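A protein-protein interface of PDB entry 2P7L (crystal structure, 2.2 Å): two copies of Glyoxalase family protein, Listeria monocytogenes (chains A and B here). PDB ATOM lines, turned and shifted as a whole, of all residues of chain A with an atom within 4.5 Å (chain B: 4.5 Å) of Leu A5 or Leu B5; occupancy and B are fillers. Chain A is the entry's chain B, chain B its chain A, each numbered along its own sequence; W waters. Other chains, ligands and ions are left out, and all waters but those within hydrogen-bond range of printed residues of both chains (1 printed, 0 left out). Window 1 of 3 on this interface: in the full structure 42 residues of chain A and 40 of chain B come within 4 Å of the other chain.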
ATOM      1  N   GLY A   4      27.871  -9.036 -24.019  1.00  0.00           N
ATOM      2  CA  GLY A   4      26.572  -9.117 -24.662  1.00  0.00           C
ATOM      3  C   GLY A   4      26.546  -9.947 -25.930  1.00  0.00           C
ATOM      4  O   GLY A   4      27.480 -10.680 -26.237  1.00  0.00           O
ATOM      5  N   LEU A   5      25.455  -9.828 -26.671  1.00  0.00           N
ATOM      6  CA  LEU A   5      25.282 -10.555 -27.914  1.00  0.00           C
ATOM      7  C   LEU A   5      26.084  -9.862 -29.010  1.00  0.00           C
ATOM      8  O   LEU A   5      26.007  -8.647 -29.151  1.00  0.00           O
ATOM      9  CB  LEU A   5      23.795 -10.567 -28.298  1.00  0.00           C
ATOM     10  CG  LEU A   5      23.364 -11.264 -29.594  1.00  0.00           C
ATOM     11  CD1 LEU A   5      23.554 -12.771 -29.477  1.00  0.00           C
ATOM     12  CD2 LEU A   5      21.915 -10.952 -29.866  1.00  0.00           C
ATOM     13  N   SER A   6      26.874 -10.618 -29.764  1.00  0.00           N
ATOM     14  CA  SER A   6      27.630 -10.031 -30.866  1.00  0.00           C
ATOM     15  C   SER A   6      26.737 -10.070 -32.103  1.00  0.00           C
ATOM     16  O   SER A   6      26.493  -9.045 -32.736  1.00  0.00           O
ATOM     17  CB  SER A   6      28.900 -10.820 -31.150  1.00  0.00           C
ATOM     18  OG  SER A   6      29.617 -10.207 -32.209  1.00  0.00           O
ATOM     19  N   HIS A   7      26.248 -11.261 -32.440  1.00  0.00           N
ATOM     20  CA  HIS A   7      25.359 -11.437 -33.587  1.00  0.00           C
ATOM     21  C   HIS A   7      24.736 -12.823 -33.620  1.00  0.00           C
ATOM     22  O   HIS A   7      25.062 -13.681 -32.801  1.00  0.00           O
ATOM     23  CB  HIS A   7      26.103 -11.202 -34.908  1.00  0.00           C
ATOM     24  CG  HIS A   7      27.238 -12.148 -35.154  1.00  0.00           C
ATOM     25  ND1 HIS A   7      28.500 -11.951 -34.635  1.00  0.00           N
ATOM     26  CD2 HIS A   7      27.317 -13.268 -35.915  1.00  0.00           C
ATOM     27  CE1 HIS A   7      29.311 -12.899 -35.074  1.00  0.00           C
ATOM     28  NE2 HIS A   7      28.619 -13.710 -35.854  1.00  0.00           N
ATOM     29  N   ILE A   8      23.836 -13.031 -34.573  1.00  0.00           N
ATOM     30  CA  ILE A   8      23.173 -14.314 -34.746  1.00  0.00           C
ATOM     31  C   ILE A   8      23.358 -14.720 -36.206  1.00  0.00           C
ATOM     32  O   ILE A   8      23.008 -13.974 -37.119  1.00  0.00           O
ATOM     33  CB  ILE A   8      21.673 -14.212 -34.423  1.00  0.00           C
ATOM     34  CG1 ILE A   8      21.495 -13.735 -32.981  1.00  0.00           C
ATOM     35  CG2 ILE A   8      21.002 -15.559 -34.627  1.00  0.00           C
ATOM     36  CD1 ILE A   8      20.074 -13.655 -32.528  1.00  0.00           C
ATOM     37  N   LEU A  52      19.872  -5.523 -33.412  1.00  0.00           N
ATOM     38  CA  LEU A  52      20.644  -6.759 -33.416  1.00  0.00           C
ATOM     39  C   LEU A  52      21.276  -7.105 -34.759  1.00  0.00           C
ATOM     40  O   LEU A  52      20.625  -7.061 -35.799  1.00  0.00           O
ATOM     41  CB  LEU A  52      19.754  -7.918 -32.976  1.00  0.00           C
ATOM     42  CG  LEU A  52      18.832  -7.594 -31.800  1.00  0.00           C
ATOM     43  CD1 LEU A  52      17.811  -8.695 -31.661  1.00  0.00           C
ATOM     44  CD2 LEU A  52      19.643  -7.421 -30.524  1.00  0.00           C
ATOM     45  N   ILE A  70      14.646 -18.726 -31.898  1.00  0.00           N
ATOM     46  CA  ILE A  70      14.957 -17.353 -31.551  1.00  0.00           C
ATOM     47  C   ILE A  70      13.632 -16.599 -31.485  1.00  0.00           C
ATOM     48  O   ILE A  70      12.796 -16.696 -32.387  1.00  0.00           O
ATOM     49  CB  ILE A  70      15.888 -16.745 -32.606  1.00  0.00           C
ATOM     50  CG1 ILE A  70      17.200 -17.538 -32.618  1.00  0.00           C
ATOM     51  CG2 ILE A  70      16.145 -15.274 -32.305  1.00  0.00           C
ATOM     52  CD1 ILE A  70      18.094 -17.288 -33.820  1.00  0.00           C
ATOM     53  N   ALA A  71      13.427 -15.865 -30.400  1.00  0.00           N
ATOM     54  CA  ALA A  71      12.188 -15.118 -30.231  1.00  0.00           C
ATOM     55  C   ALA A  71      12.416 -13.618 -30.227  1.00  0.00           C
ATOM     56  O   ALA A  71      13.279 -13.106 -29.508  1.00  0.00           O
ATOM     57  CB  ALA A  71      11.499 -15.531 -28.940  1.00  0.00           C
ATOM     58  N   GLN A  73      10.779  -9.714 -29.771  1.00  0.00           N
ATOM     59  CA  GLN A  73       9.746  -9.069 -28.977  1.00  0.00           C
ATOM     60  C   GLN A  73       8.909  -8.047 -29.743  1.00  0.00           C
ATOM     61  O   GLN A  73       9.418  -7.333 -30.604  1.00  0.00           O
ATOM     62  CB  GLN A  73      10.387  -8.406 -27.749  1.00  0.00           C
ATOM     63  CG  GLN A  73       9.449  -7.502 -26.968  1.00  0.00           C
ATOM     64  CD  GLN A  73       9.816  -7.403 -25.502  1.00  0.00           C
ATOM     65  OE1 GLN A  73      10.950  -7.069 -25.147  1.00  0.00           O
ATOM     66  NE2 GLN A  73       8.850  -7.691 -24.637  1.00  0.00           N
ATOM     67  N   GLY B   4      13.052  -5.638 -30.218  1.00  0.00           N
ATOM     68  CA  GLY B   4      14.378  -6.186 -30.011  1.00  0.00           C
ATOM     69  C   GLY B   4      14.283  -7.679 -29.763  1.00  0.00           C
ATOM     70  O   GLY B   4      13.270  -8.309 -30.079  1.00  0.00           O
ATOM     71  N   LEU B   5      15.335  -8.248 -29.192  1.00  0.00           N
ATOM     72  CA  LEU B   5      15.366  -9.676 -28.903  1.00  0.00           C
ATOM     73  C   LEU B   5      14.638  -9.986 -27.594  1.00  0.00           C
ATOM     74  O   LEU B   5      14.887  -9.343 -26.578  1.00  0.00           O
ATOM     75  CB  LEU B   5      16.822 -10.138 -28.813  1.00  0.00           C
ATOM     76  CG  LEU B   5      17.169 -11.612 -28.605  1.00  0.00           C
ATOM     77  CD1 LEU B   5      16.662 -12.441 -29.768  1.00  0.00           C
ATOM     78  CD2 LEU B   5      18.684 -11.747 -28.488  1.00  0.00           C
ATOM     79  N   SER B   6      13.723 -10.948 -27.625  1.00  0.00           N
ATOM     80  CA  SER B   6      13.004 -11.341 -26.414  1.00  0.00           C
ATOM     81  C   SER B   6      13.838 -12.362 -25.646  1.00  0.00           C
ATOM     82  O   SER B   6      14.221 -12.130 -24.498  1.00  0.00           O
ATOM     83  CB  SER B   6      11.655 -11.979 -26.746  1.00  0.00           C
ATOM     84  OG  SER B   6      11.039 -12.475 -25.565  1.00  0.00           O
ATOM     85  N   HIS B   7      14.124 -13.488 -26.297  1.00  0.00           N
ATOM     86  CA  HIS B   7      14.906 -14.555 -25.684  1.00  0.00           C
ATOM     87  C   HIS B   7      15.263 -15.642 -26.687  1.00  0.00           C
ATOM     88  O   HIS B   7      14.664 -15.742 -27.758  1.00  0.00           O
ATOM     89  CB  HIS B   7      14.110 -15.206 -24.561  1.00  0.00           C
ATOM     90  CG  HIS B   7      12.845 -15.857 -25.027  1.00  0.00           C
ATOM     91  ND1 HIS B   7      11.668 -15.162 -25.199  1.00  0.00           N
ATOM     92  CD2 HIS B   7      12.586 -17.133 -25.400  1.00  0.00           C
ATOM     93  CE1 HIS B   7      10.737 -15.982 -25.654  1.00  0.00           C
ATOM     94  NE2 HIS B   7      11.267 -17.183 -25.785  1.00  0.00           N
ATOM     95  N   ILE B   8      16.232 -16.469 -26.315  1.00  0.00           N
ATOM     96  CA  ILE B   8      16.663 -17.580 -27.147  1.00  0.00           C
ATOM     97  C   ILE B   8      16.331 -18.880 -26.404  1.00  0.00           C
ATOM     98  O   ILE B   8      16.599 -19.012 -25.209  1.00  0.00           O
ATOM     99  CB  ILE B   8      18.178 -17.506 -27.427  1.00  0.00           C
ATOM    100  CG1 ILE B   8      18.494 -16.217 -28.186  1.00  0.00           C
ATOM    101  CG2 ILE B   8      18.622 -18.715 -28.228  1.00  0.00           C
ATOM    102  CD1 ILE B   8      19.962 -15.954 -28.368  1.00  0.00           C
ATOM    103  N   LEU B  52      21.019 -11.171 -21.820  1.00  0.00           N
ATOM    104  CA  LEU B  52      20.125 -11.939 -22.680  1.00  0.00           C
ATOM    105  C   LEU B  52      19.378 -13.050 -21.937  1.00  0.00           C
ATOM    106  O   LEU B  52      19.982 -13.843 -21.212  1.00  0.00           O
ATOM    107  CB  LEU B  52      20.936 -12.544 -23.825  1.00  0.00           C
ATOM    108  CG  LEU B  52      21.948 -11.549 -24.411  1.00  0.00           C
ATOM    109  CD1 LEU B  52      23.037 -12.293 -25.165  1.00  0.00           C
ATOM    110  CD2 LEU B  52      21.223 -10.539 -25.311  1.00  0.00           C
ATOM    111  N   ALA B  71      26.467 -15.742 -31.289  1.00  0.00           N
ATOM    112  CA  ALA B  71      27.813 -15.372 -30.889  1.00  0.00           C
ATOM    113  C   ALA B  71      27.722 -14.276 -29.834  1.00  0.00           C
ATOM    114  O   ALA B  71      26.885 -13.376 -29.937  1.00  0.00           O
ATOM    115  CB  ALA B  71      28.596 -14.885 -32.096  1.00  0.00           C
ATOM    116  N   PHE B  72      28.568 -14.360 -28.811  1.00  0.00           N
ATOM    117  CA  PHE B  72      28.570 -13.347 -27.759  1.00  0.00           C
ATOM    118  C   PHE B  72      29.805 -12.471 -27.909  1.00  0.00           C
ATOM    119  O   PHE B  72      30.837 -12.901 -28.435  1.00  0.00           O
ATOM    120  CB  PHE B  72      28.590 -13.967 -26.360  1.00  0.00           C
ATOM    121  CG  PHE B  72      27.381 -14.789 -26.029  1.00  0.00           C
ATOM    122  CD1 PHE B  72      27.366 -16.160 -26.277  1.00  0.00           C
ATOM    123  CD2 PHE B  72      26.273 -14.205 -25.441  1.00  0.00           C
ATOM    124  CE1 PHE B  72      26.264 -16.934 -25.940  1.00  0.00           C
ATOM    125  CE2 PHE B  72      25.164 -14.970 -25.098  1.00  0.00           C
ATOM    126  CZ  PHE B  72      25.165 -16.340 -25.350  1.00  0.00           C
ATOM    127  N   GLN B  73      29.698 -11.244 -27.426  1.00  0.00           N
ATOM    128  CA  GLN B  73      30.794 -10.307 -27.511  1.00  0.00           C
ATOM    129  C   GLN B  73      31.745 -10.382 -26.320  1.00  0.00           C
ATOM    130  O   GLN B  73      31.311 -10.357 -25.166  1.00  0.00           O
ATOM    131  CB  GLN B  73      30.236  -8.884 -27.618  1.00  0.00           C
ATOM    132  CG  GLN B  73      31.292  -7.799 -27.750  1.00  0.00           C
ATOM    133  CD  GLN B  73      31.738  -7.599 -29.183  1.00  0.00           C
ATOM    134  OE1 GLN B  73      30.912  -7.376 -30.072  1.00  0.00           O
ATOM    135  NE2 GLN B  73      33.049  -7.666 -29.418  1.00  0.00           N
HETATM  136  O   HOH W   1      30.285  -7.628 -32.637  1.00  0.00           O
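O of Gly B4 sits at hydrogen-bond distance from N of Gln A73 (2.9 Å). The backbone carbonyl oxygen (O) of Ala A71 is in hydrogen-bond range of the backbone NH (N) of Ser B6 (2.9 Å). O of His B7 sits at hydrogen-bond distance from N of Ala A71 (2.9 Å). The backbone carbonyl oxygen (O) of Ala B71 sits at hydrogen-bond distance from the backbone NH (N) of Ser A6 (2.8 Å). The backbone carbonyl oxygen of His A7 is in hydrogen-bond range of the backbone NH of Ala B71, at 2.9 Å. The backbone NH of Gln B73 is in hydrogen-bond range of the backbone carbonyl oxygen of Gly A4 (2.6 Å).
A ring nitrogen (ND1) of His B7 lies within hydrogen-bond range of the side-chain hydroxyl (OG) of Ser B6 (2.8 Å). OG of Ser A6 is in hydrogen-bond range of ND1 of His A7, 3.2 Å away.
Among the printed residues, merely in contact across the chains: Gly A4 with Phe B72 (3.3 Å), Leu A52 with Leu B5 (3.3 Å), Leu A5 with Ala B71 (3.4 Å), Ala A71 with Leu B5 (3.5 Å), Leu A5 with Leu B5 (3.6 Å), Leu A5 with Leu B52 (3.7 Å), Ser A6 with Gln B73 (3.7 Å), Ser A6 with Phe B72 (3.7 Å), Ile A70 with Leu B5 (3.8 Å), Gln A73 with Ser B6 (3.8 Å) and Ile A70 with His B7 (3.96 Å).
Printed residues of chain B within 4 Å of Ile A70: Leu B5 and His B7. Of chain A, only Leu A5, Leu A52, Ile A70 and Ala A71 come within 4 Å of Leu B5. Of the printed residues of chain A, Ser B6 touches Ala A71 (2.9 Å) and Gln A73 (3.8 Å). The nearest residue of chain A that does not touch Leu B5 is Gln A73 (4.4 Å).
Of the 9 printed residues of chain B, 8 touch a printed residue of chain A. Hydrophobic or aromatic side chains of chain B that line the printed part of chain A: Leu B5, His B7, Leu B52, Ala B71 and Phe B72. Printed residues of chain A that touch a printed residue of chain B: Gly A4, Leu A5, Ser A6, His A7, Leu A52, Ile A70, Ala A71 and Gln A73. Among the printed residues, 17 pairs touch across the chains.
Gly A4 touches Gln B73, and with the chains exchanged Gln A73 touches Gly B4. Leu A5 touches Leu B52, and with the chains exchanged Leu A52 touches Leu B5. Ser A6 touches Ala B71, and with the chains exchanged Ala A71 touches Ser B6. His A7 touches Ala B71, and with the chains exchanged Ala A71 touches His B7. Of the 17 pairs that touch across the chains among the printed residues, 13 have their exchanged pair printed and touching as well.
Water W1 bridges the side-chain amide oxygen (OE1) of Gln B73 and the side-chain hydroxyl (OG) of Ser A6.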
